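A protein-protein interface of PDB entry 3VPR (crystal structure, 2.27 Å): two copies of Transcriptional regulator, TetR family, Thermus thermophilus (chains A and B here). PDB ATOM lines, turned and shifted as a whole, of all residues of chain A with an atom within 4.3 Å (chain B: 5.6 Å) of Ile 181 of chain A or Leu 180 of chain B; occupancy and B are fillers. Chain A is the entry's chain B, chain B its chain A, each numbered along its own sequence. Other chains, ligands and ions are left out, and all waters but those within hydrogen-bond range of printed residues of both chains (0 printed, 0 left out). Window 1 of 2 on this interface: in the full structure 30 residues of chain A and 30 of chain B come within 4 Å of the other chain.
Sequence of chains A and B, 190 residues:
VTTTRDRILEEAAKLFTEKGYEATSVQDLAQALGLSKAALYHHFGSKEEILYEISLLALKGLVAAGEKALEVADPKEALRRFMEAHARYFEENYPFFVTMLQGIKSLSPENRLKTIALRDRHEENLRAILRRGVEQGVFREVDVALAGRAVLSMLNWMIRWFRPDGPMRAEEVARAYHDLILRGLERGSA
The backbone carbonyl oxygen (O) of Gly 184 of chain B is in hydrogen-bond range of the guanidinium group (NH2) of Arg 140 of chain A, 2.9 Å away.
The guanidinium group (NH1) of Arg 140 of chain A lies close to the guanidinium group (NH1) of Arg 183 of chain B, at 3.5 Å.
The backbone NH (N) of Leu 185 of chain B is in hydrogen-bond range of the backbone carbonyl oxygen (O) of Leu 182 of chain A, at 3.0 Å.
O of Leu 185 of chain B sits at hydrogen-bond distance from N of Arg 140 of chain A, 2.5 Å away.
The backbone NH (N) of Leu 185 of chain B sits at hydrogen-bond distance from the backbone carbonyl oxygen (O) of Ile 181 of chain A, at 2.9 Å.
O of Arg 183 of chain A lies close to O of Arg 183 of chain B, 3.3 Å away.
The backbone NH (N) of Glu 186 of chain B sits at hydrogen-bond distance from the backbone carbonyl oxygen (O) of Leu 182 of chain A (3.0 Å).
NH1 of Arg 140 of chain A is in salt-bridge range of OD2 of Asp 179 of chain B, at 3.2 Å.
The side-chain carboxylate (OD1) of Asp 179 of chain B lies within salt-bridge range of the guanidinium group (NH1) of Arg 183 of chain B (3.3 Å).
The side-chain carboxylate of Asp 179 of chain A is in salt-bridge range of the guanidinium group of Arg 183 of chain A, 3.3 Å away.
Among the printed residues, pairs that only touch across the chains: Arg 140 of chain A with Glu 186 of chain B, Ala 147 of chain A with Leu 180 of chain B, Ala 150 of chain A with Tyr 177 of chain B, Ala 150 of chain A with Leu 180 of chain B, Leu 180 of chain A with Ile 181 of chain B, Ile 181 of chain A with Leu 180 of chain B, Ile 181 of chain A with Gly 184 of chain B, Leu 182 of chain A with Gly 184 of chain B, Arg 183 of chain A with Gly 184 of chain B, Arg 183 of chain A with Glu 186 of chain B, Gly 184 of chain A with Ile 181 of chain B, Gly 184 of chain A with Leu 182 of chain B, Gly 184 of chain A with Arg 183 of chain B and Gly 184 of chain A with Gly 184 of chain B.
Of the printed residues of chain B, Leu 180 of chain A touches Ile 181.
Of chain B, only Leu 180 (3.5 Å), Gly 184 (3.4 Å) and Leu 185 (2.9 Å) come within 4 Å of Ile 181 of chain A.
Printed residues of chain B within 4 Å of Leu 182 of chain A: Gly 184, Leu 185 and Glu 186.
Of the printed residues of chain A, Tyr 177 of chain B touches Ala 150.
Leu 180 of chain B touches just these residues of chain A: Ala 147, Ala 150 and Ile 181.
Printed residues of chain A within 4 Å of Arg 183 of chain B: Arg 140 (3.4 Å), Arg 183 (3.3 Å) and Gly 184 (3.8 Å).
The nearest residue of chain B that does not touch Ile 181 of chain A is Ile 181 of chain B (4.8 Å).
The nearest printed residue of chain A that does not touch Ile 181 of chain B is Ile 181 of chain A (4.8 Å).
Among the printed residues, Asp or Glu carboxylates within 4 Å of a Lys or Arg side-chain nitrogen of the other chain: Arg 140 of chain A with Asp 179 of chain B (3.2 Å).
Leu 180 of chain A touches Ile 181 of chain B, and with the chains exchanged Ile 181 of chain A touches Leu 180 of chain B.
Ile 181 of chain A touches Gly 184 of chain B, and with the chains exchanged Gly 184 of chain A touches Ile 181 of chain B.
Leu 182 of chain A touches Gly 184 of chain B, and with the chains exchanged Gly 184 of chain A touches Leu 182 of chain B.
Arg 183 of chain B touches its own counterpart, Arg 183 of chain A.
Of the 22 pairs that touch across the chains among the printed residues, 10 have their exchanged pair printed and touching as well.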
ATOM      1  N   ARG A 140      17.241 -33.798 -19.546  1.00  0.00           N
ATOM      2  CA  ARG A 140      18.003 -33.019 -20.516  1.00  0.00           C
ATOM      3  C   ARG A 140      19.431 -33.567 -20.487  1.00  0.00           C
ATOM      4  O   ARG A 140      19.845 -34.189 -19.497  1.00  0.00           O
ATOM      5  CB  ARG A 140      17.976 -31.546 -20.086  1.00  0.00           C
ATOM      6  CG  ARG A 140      18.714 -30.565 -20.968  1.00  0.00           C
ATOM      7  CD  ARG A 140      18.319 -29.138 -20.577  1.00  0.00           C
ATOM      8  NE  ARG A 140      18.609 -28.845 -19.175  1.00  0.00           N
ATOM      9  CZ  ARG A 140      19.717 -28.245 -18.751  1.00  0.00           C
ATOM     10  NH1 ARG A 140      20.643 -27.861 -19.621  1.00  0.00           N
ATOM     11  NH2 ARG A 140      19.910 -28.040 -17.453  1.00  0.00           N
ATOM     12  N   ALA A 147      25.866 -33.544 -12.170  1.00  0.00           N
ATOM     13  CA  ALA A 147      24.487 -33.588 -11.698  1.00  0.00           C
ATOM     14  C   ALA A 147      24.413 -34.453 -10.433  1.00  0.00           C
ATOM     15  O   ALA A 147      23.767 -34.083  -9.460  1.00  0.00           O
ATOM     16  CB  ALA A 147      23.580 -34.153 -12.784  1.00  0.00           C
ATOM     17  N   ALA A 150      25.902 -32.738  -7.558  1.00  0.00           N
ATOM     18  CA  ALA A 150      25.027 -31.662  -7.131  1.00  0.00           C
ATOM     19  C   ALA A 150      23.947 -32.205  -6.200  1.00  0.00           C
ATOM     20  O   ALA A 150      23.712 -31.654  -5.117  1.00  0.00           O
ATOM     21  CB  ALA A 150      24.401 -30.974  -8.344  1.00  0.00           C
ATOM     22  N   MET A 154      23.454 -31.583  -2.013  1.00  0.00           N
ATOM     23  CA  MET A 154      22.226 -31.155  -1.361  1.00  0.00           C
ATOM     24  C   MET A 154      21.829 -32.090  -0.211  1.00  0.00           C
ATOM     25  O   MET A 154      21.390 -31.642   0.852  1.00  0.00           O
ATOM     26  CB  MET A 154      21.085 -31.107  -2.381  1.00  0.00           C
ATOM     27  CG  MET A 154      21.122 -29.908  -3.341  1.00  0.00           C
ATOM     28  SD  MET A 154      19.724 -30.046  -4.697  1.00  0.00           S
ATOM     29  CE  MET A 154      20.870 -30.375  -6.203  1.00  0.00           C
ATOM     30  N   TYR A 177      13.906 -30.561  -2.656  1.00  0.00           N
ATOM     31  CA  TYR A 177      15.153 -30.456  -3.403  1.00  0.00           C
ATOM     32  C   TYR A 177      14.974 -31.107  -4.770  1.00  0.00           C
ATOM     33  O   TYR A 177      15.523 -30.624  -5.766  1.00  0.00           O
ATOM     34  CB  TYR A 177      16.304 -31.148  -2.672  1.00  0.00           C
ATOM     35  CG  TYR A 177      16.937 -30.345  -1.555  1.00  0.00           C
ATOM     36  CD1 TYR A 177      16.860 -28.957  -1.537  1.00  0.00           C
ATOM     37  CD2 TYR A 177      17.700 -30.976  -0.573  1.00  0.00           C
ATOM     38  CE1 TYR A 177      17.545 -28.205  -0.571  1.00  0.00           C
ATOM     39  CE2 TYR A 177      18.383 -30.244   0.399  1.00  0.00           C
ATOM     40  CZ  TYR A 177      18.308 -28.861   0.391  1.00  0.00           C
ATOM     41  OH  TYR A 177      19.035 -28.133   1.311  1.00  0.00           O
ATOM     42  N   HIS A 178      14.207 -32.201  -4.805  1.00  0.00           N
ATOM     43  CA  HIS A 178      13.947 -32.938  -6.038  1.00  0.00           C
ATOM     44  C   HIS A 178      13.150 -32.074  -7.013  1.00  0.00           C
ATOM     45  O   HIS A 178      13.478 -31.995  -8.194  1.00  0.00           O
ATOM     46  CB  HIS A 178      13.176 -34.239  -5.746  1.00  0.00           C
ATOM     47  CG  HIS A 178      12.737 -34.964  -6.979  1.00  0.00           C
ATOM     48  ND1 HIS A 178      11.474 -34.822  -7.512  1.00  0.00           N
ATOM     49  CD2 HIS A 178      13.413 -35.782  -7.823  1.00  0.00           C
ATOM     50  CE1 HIS A 178      11.389 -35.518  -8.632  1.00  0.00           C
ATOM     51  NE2 HIS A 178      12.551 -36.111  -8.845  1.00  0.00           N
ATOM     52  N   ASP A 179      12.091 -31.450  -6.510  1.00  0.00           N
ATOM     53  CA  ASP A 179      11.271 -30.564  -7.324  1.00  0.00           C
ATOM     54  C   ASP A 179      12.168 -29.463  -7.897  1.00  0.00           C
ATOM     55  O   ASP A 179      12.088 -29.139  -9.078  1.00  0.00           O
ATOM     56  CB  ASP A 179      10.175 -29.910  -6.479  1.00  0.00           C
ATOM     57  CG  ASP A 179       9.491 -28.762  -7.207  1.00  0.00           C
ATOM     58  OD1 ASP A 179       8.680 -29.045  -8.114  1.00  0.00           O
ATOM     59  OD2 ASP A 179       9.778 -27.582  -6.885  1.00  0.00           O
ATOM     60  N   LEU A 180      13.025 -28.905  -7.046  1.00  0.00           N
ATOM     61  CA  LEU A 180      13.928 -27.845  -7.455  1.00  0.00           C
ATOM     62  C   LEU A 180      14.928 -28.282  -8.518  1.00  0.00           C
ATOM     63  O   LEU A 180      15.056 -27.624  -9.548  1.00  0.00           O
ATOM     64  CB  LEU A 180      14.672 -27.288  -6.238  1.00  0.00           C
ATOM     65  CG  LEU A 180      15.677 -26.163  -6.521  1.00  0.00           C
ATOM     66  CD1 LEU A 180      14.984 -25.021  -7.287  1.00  0.00           C
ATOM     67  CD2 LEU A 180      16.260 -25.651  -5.217  1.00  0.00           C
ATOM     68  N   ILE A 181      15.616 -29.399  -8.290  1.00  0.00           N
ATOM     69  CA  ILE A 181      16.614 -29.886  -9.252  1.00  0.00           C
ATOM     70  C   ILE A 181      16.000 -30.416 -10.550  1.00  0.00           C
ATOM     71  O   ILE A 181      16.616 -30.367 -11.603  1.00  0.00           O
ATOM     72  CB  ILE A 181      17.509 -31.008  -8.634  1.00  0.00           C
ATOM     73  CG1 ILE A 181      18.741 -31.247  -9.513  1.00  0.00           C
ATOM     74  CG2 ILE A 181      16.751 -32.299  -8.531  1.00  0.00           C
ATOM     75  CD1 ILE A 181      19.669 -30.043  -9.590  1.00  0.00           C
ATOM     76  N   LEU A 182      14.786 -30.934 -10.477  1.00  0.00           N
ATOM     77  CA  LEU A 182      14.148 -31.462 -11.676  1.00  0.00           C
ATOM     78  C   LEU A 182      13.627 -30.353 -12.595  1.00  0.00           C
ATOM     79  O   LEU A 182      13.890 -30.347 -13.790  1.00  0.00           O
ATOM     80  CB  LEU A 182      12.988 -32.384 -11.285  1.00  0.00           C
ATOM     81  CG  LEU A 182      12.146 -32.950 -12.426  1.00  0.00           C
ATOM     82  CD1 LEU A 182      13.018 -33.854 -13.274  1.00  0.00           C
ATOM     83  CD2 LEU A 182      10.936 -33.716 -11.861  1.00  0.00           C
ATOM     84  N   ARG A 183      12.906 -29.404 -12.019  1.00  0.00           N
ATOM     85  CA  ARG A 183      12.308 -28.338 -12.793  1.00  0.00           C
ATOM     86  C   ARG A 183      13.144 -27.073 -12.938  1.00  0.00           C
ATOM     87  O   ARG A 183      12.903 -26.267 -13.835  1.00  0.00           O
ATOM     88  CB  ARG A 183      10.943 -28.019 -12.184  1.00  0.00           C
ATOM     89  CG  ARG A 183      10.072 -29.275 -12.058  1.00  0.00           C
ATOM     90  CD  ARG A 183       8.738 -29.016 -11.394  1.00  0.00           C
ATOM     91  NE  ARG A 183       7.770 -30.071 -11.704  1.00  0.00           N
ATOM     92  CZ  ARG A 183       7.722 -31.269 -11.118  1.00  0.00           C
ATOM     93  NH1 ARG A 183       8.584 -31.598 -10.163  1.00  0.00           N
ATOM     94  NH2 ARG A 183       6.806 -32.148 -11.502  1.00  0.00           N
ATOM     95  N   GLY A 184      14.138 -26.908 -12.076  1.00  0.00           N
ATOM     96  CA  GLY A 184      14.956 -25.715 -12.143  1.00  0.00           C
ATOM     97  C   GLY A 184      14.227 -24.531 -11.531  1.00  0.00           C
ATOM     98  O   GLY A 184      13.122 -24.671 -11.006  1.00  0.00           O
ATOM     99  N   MET B 154      25.636 -26.853  -2.825  1.00  0.00           N
ATOM    100  CA  MET B 154      26.467 -27.224  -3.965  1.00  0.00           C
ATOM    101  C   MET B 154      27.846 -26.560  -3.869  1.00  0.00           C
ATOM    102  O   MET B 154      28.878 -27.211  -4.045  1.00  0.00           O
ATOM    103  CB  MET B 154      25.785 -26.835  -5.283  1.00  0.00           C
ATOM    104  CG  MET B 154      24.503 -27.607  -5.581  1.00  0.00           C
ATOM    105  SD  MET B 154      23.556 -26.933  -7.143  1.00  0.00           S
ATOM    106  CE  MET B 154      22.311 -25.755  -6.302  1.00  0.00           C
ATOM    107  N   ARG B 175      29.639 -22.915 -12.786  1.00  0.00           N
ATOM    108  CA  ARG B 175      28.848 -22.504 -13.940  1.00  0.00           C
ATOM    109  C   ARG B 175      27.921 -23.633 -14.383  1.00  0.00           C
ATOM    110  O   ARG B 175      26.773 -23.392 -14.770  1.00  0.00           O
ATOM    111  CB  ARG B 175      29.753 -22.076 -15.098  1.00  0.00           C
ATOM    112  CG  ARG B 175      28.985 -21.523 -16.280  1.00  0.00           C
ATOM    113  CD  ARG B 175      29.903 -20.782 -17.232  1.00  0.00           C
ATOM    114  NE  ARG B 175      30.611 -19.694 -16.561  1.00  0.00           N
ATOM    115  CZ  ARG B 175      31.419 -18.833 -17.173  1.00  0.00           C
ATOM    116  NH1 ARG B 175      32.021 -17.877 -16.480  1.00  0.00           N
ATOM    117  NH2 ARG B 175      31.620 -18.924 -18.482  1.00  0.00           N
ATOM    118  N   ALA B 176      28.426 -24.862 -14.324  1.00  0.00           N
ATOM    119  CA  ALA B 176      27.624 -26.021 -14.696  1.00  0.00           C
ATOM    120  C   ALA B 176      26.508 -26.194 -13.663  1.00  0.00           C
ATOM    121  O   ALA B 176      25.392 -26.580 -14.011  1.00  0.00           O
ATOM    122  CB  ALA B 176      28.491 -27.270 -14.759  1.00  0.00           C
ATOM    123  N   TYR B 177      26.805 -25.894 -12.395  1.00  0.00           N
ATOM    124  CA  TYR B 177      25.794 -25.999 -11.339  1.00  0.00           C
ATOM    125  C   TYR B 177      24.707 -24.951 -11.570  1.00  0.00           C
ATOM    126  O   TYR B 177      23.516 -25.203 -11.342  1.00  0.00           O
ATOM    127  CB  TYR B 177      26.407 -25.772  -9.950  1.00  0.00           C
ATOM    128  CG  TYR B 177      27.152 -26.953  -9.365  1.00  0.00           C
ATOM    129  CD1 TYR B 177      26.839 -28.261  -9.731  1.00  0.00           C
ATOM    130  CD2 TYR B 177      28.121 -26.763  -8.390  1.00  0.00           C
ATOM    131  CE1 TYR B 177      27.472 -29.345  -9.131  1.00  0.00           C
ATOM    132  CE2 TYR B 177      28.756 -27.837  -7.783  1.00  0.00           C
ATOM    133  CZ  TYR B 177      28.426 -29.124  -8.153  1.00  0.00           C
ATOM    134  OH  TYR B 177      29.022 -30.184  -7.506  1.00  0.00           O
ATOM    135  N   HIS B 178      25.116 -23.772 -12.033  1.00  0.00           N
ATOM    136  CA  HIS B 178      24.155 -22.702 -12.281  1.00  0.00           C
ATOM    137  C   HIS B 178      23.189 -23.089 -13.388  1.00  0.00           C
ATOM    138  O   HIS B 178      21.974 -22.871 -13.277  1.00  0.00           O
ATOM    139  CB  HIS B 178      24.867 -21.395 -12.641  1.00  0.00           C
ATOM    140  CG  HIS B 178      23.934 -20.322 -13.102  1.00  0.00           C
ATOM    141  ND1 HIS B 178      23.648 -20.107 -14.432  1.00  0.00           N
ATOM    142  CD2 HIS B 178      23.169 -19.447 -12.407  1.00  0.00           C
ATOM    143  CE1 HIS B 178      22.749 -19.146 -14.538  1.00  0.00           C
ATOM    144  NE2 HIS B 178      22.438 -18.729 -13.323  1.00  0.00           N
ATOM    145  N   ASP B 179      23.738 -23.657 -14.458  1.00  0.00           N
ATOM    146  CA  ASP B 179      22.918 -24.096 -15.578  1.00  0.00           C
ATOM    147  C   ASP B 179      21.940 -25.150 -15.073  1.00  0.00           C
ATOM    148  O   ASP B 179      20.746 -25.126 -15.401  1.00  0.00           O
ATOM    149  CB  ASP B 179      23.785 -24.707 -16.687  1.00  0.00           C
ATOM    150  CG  ASP B 179      22.950 -25.465 -17.720  1.00  0.00           C
ATOM    151  OD1 ASP B 179      22.247 -24.824 -18.526  1.00  0.00           O
ATOM    152  OD2 ASP B 179      22.978 -26.712 -17.714  1.00  0.00           O
ATOM    153  N   LEU B 180      22.448 -26.065 -14.255  1.00  0.00           N
ATOM    154  CA  LEU B 180      21.614 -27.143 -13.725  1.00  0.00           C
ATOM    155  C   LEU B 180      20.488 -26.643 -12.834  1.00  0.00           C
ATOM    156  O   LEU B 180      19.343 -27.041 -13.002  1.00  0.00           O
ATOM    157  CB  LEU B 180      22.476 -28.145 -12.944  1.00  0.00           C
ATOM    158  CG  LEU B 180      21.744 -29.338 -12.325  1.00  0.00           C
ATOM    159  CD1 LEU B 180      20.984 -30.112 -13.407  1.00  0.00           C
ATOM    160  CD2 LEU B 180      22.751 -30.248 -11.632  1.00  0.00           C
ATOM    161  N   ILE B 181      20.807 -25.760 -11.896  1.00  0.00           N
ATOM    162  CA  ILE B 181      19.801 -25.257 -10.969  1.00  0.00           C
ATOM    163  C   ILE B 181      18.825 -24.301 -11.648  1.00  0.00           C
ATOM    164  O   ILE B 181      17.648 -24.247 -11.291  1.00  0.00           O
ATOM    165  CB  ILE B 181      20.470 -24.552  -9.737  1.00  0.00           C
ATOM    166  CG1 ILE B 181      19.436 -24.327  -8.631  1.00  0.00           C
ATOM    167  CG2 ILE B 181      21.068 -23.206 -10.141  1.00  0.00           C
ATOM    168  CD1 ILE B 181      18.913 -25.602  -8.025  1.00  0.00           C
ATOM    169  N   LEU B 182      19.300 -23.554 -12.636  1.00  0.00           N
ATOM    170  CA  LEU B 182      18.415 -22.619 -13.326  1.00  0.00           C
ATOM    171  C   LEU B 182      17.405 -23.318 -14.238  1.00  0.00           C
ATOM    172  O   LEU B 182      16.212 -23.059 -14.158  1.00  0.00           O
ATOM    173  CB  LEU B 182      19.233 -21.629 -14.159  1.00  0.00           C
ATOM    174  CG  LEU B 182      18.446 -20.623 -14.998  1.00  0.00           C
ATOM    175  CD1 LEU B 182      17.686 -19.670 -14.094  1.00  0.00           C
ATOM    176  CD2 LEU B 182      19.414 -19.840 -15.892  1.00  0.00           C
ATOM    177  N   ARG B 183      17.894 -24.216 -15.087  1.00  0.00           N
ATOM    178  CA  ARG B 183      17.045 -24.917 -16.050  1.00  0.00           C
ATOM    179  C   ARG B 183      16.435 -26.246 -15.584  1.00  0.00           C
ATOM    180  O   ARG B 183      15.353 -26.630 -16.048  1.00  0.00           O
ATOM    181  CB  ARG B 183      17.839 -25.135 -17.343  1.00  0.00           C
ATOM    182  CG  ARG B 183      18.430 -23.841 -17.910  1.00  0.00           C
ATOM    183  CD  ARG B 183      19.428 -24.108 -19.033  1.00  0.00           C
ATOM    184  NE  ARG B 183      18.824 -24.837 -20.148  1.00  0.00           N
ATOM    185  CZ  ARG B 183      19.469 -25.183 -21.259  1.00  0.00           C
ATOM    186  NH1 ARG B 183      20.750 -24.863 -21.415  1.00  0.00           N
ATOM    187  NH2 ARG B 183      18.833 -25.860 -22.211  1.00  0.00           N
ATOM    188  N   GLY B 184      17.114 -26.950 -14.684  1.00  0.00           N
ATOM    189  CA  GLY B 184      16.573 -28.212 -14.201  1.00  0.00           C
ATOM    190  C   GLY B 184      17.065 -29.397 -15.004  1.00  0.00           C
ATOM    191  O   GLY B 184      17.701 -29.226 -16.057  1.00  0.00           O
ATOM    192  N   LEU B 185      16.781 -30.600 -14.514  1.00  0.00           N
ATOM    193  CA  LEU B 185      17.206 -31.827 -15.194  1.00  0.00           C
ATOM    194  C   LEU B 185      16.243 -32.267 -16.281  1.00  0.00           C
ATOM    195  O   LEU B 185      16.651 -32.836 -17.290  1.00  0.00           O
ATOM    196  CB  LEU B 185      17.343 -32.989 -14.206  1.00  0.00           C
ATOM    197  CG  LEU B 185      18.634 -33.157 -13.417  1.00  0.00           C
ATOM    198  CD1 LEU B 185      18.450 -34.298 -12.426  1.00  0.00           C
ATOM    199  CD2 LEU B 185      19.799 -33.438 -14.371  1.00  0.00           C
ATOM    200  N   GLU B 186      14.960 -32.026 -16.056  1.00  0.00           N
ATOM    201  CA  GLU B 186      13.936 -32.437 -17.008  1.00  0.00           C
ATOM    202  C   GLU B 186      14.161 -31.866 -18.393  1.00  0.00           C
ATOM    203  O   GLU B 186      14.622 -30.737 -18.543  1.00  0.00           O
ATOM    204  CB  GLU B 186      12.557 -31.998 -16.520  1.00  0.00           C
ATOM    205  CG  GLU B 186      12.354 -30.495 -16.575  1.00  0.00           C
ATOM    206  CD  GLU B 186      10.982 -30.079 -16.085  1.00  0.00           C
ATOM    207  OE1 GLU B 186      10.707 -28.858 -16.061  1.00  0.00           O
ATOM    208  OE2 GLU B 186      10.185 -30.975 -15.720  1.00  0.00           O
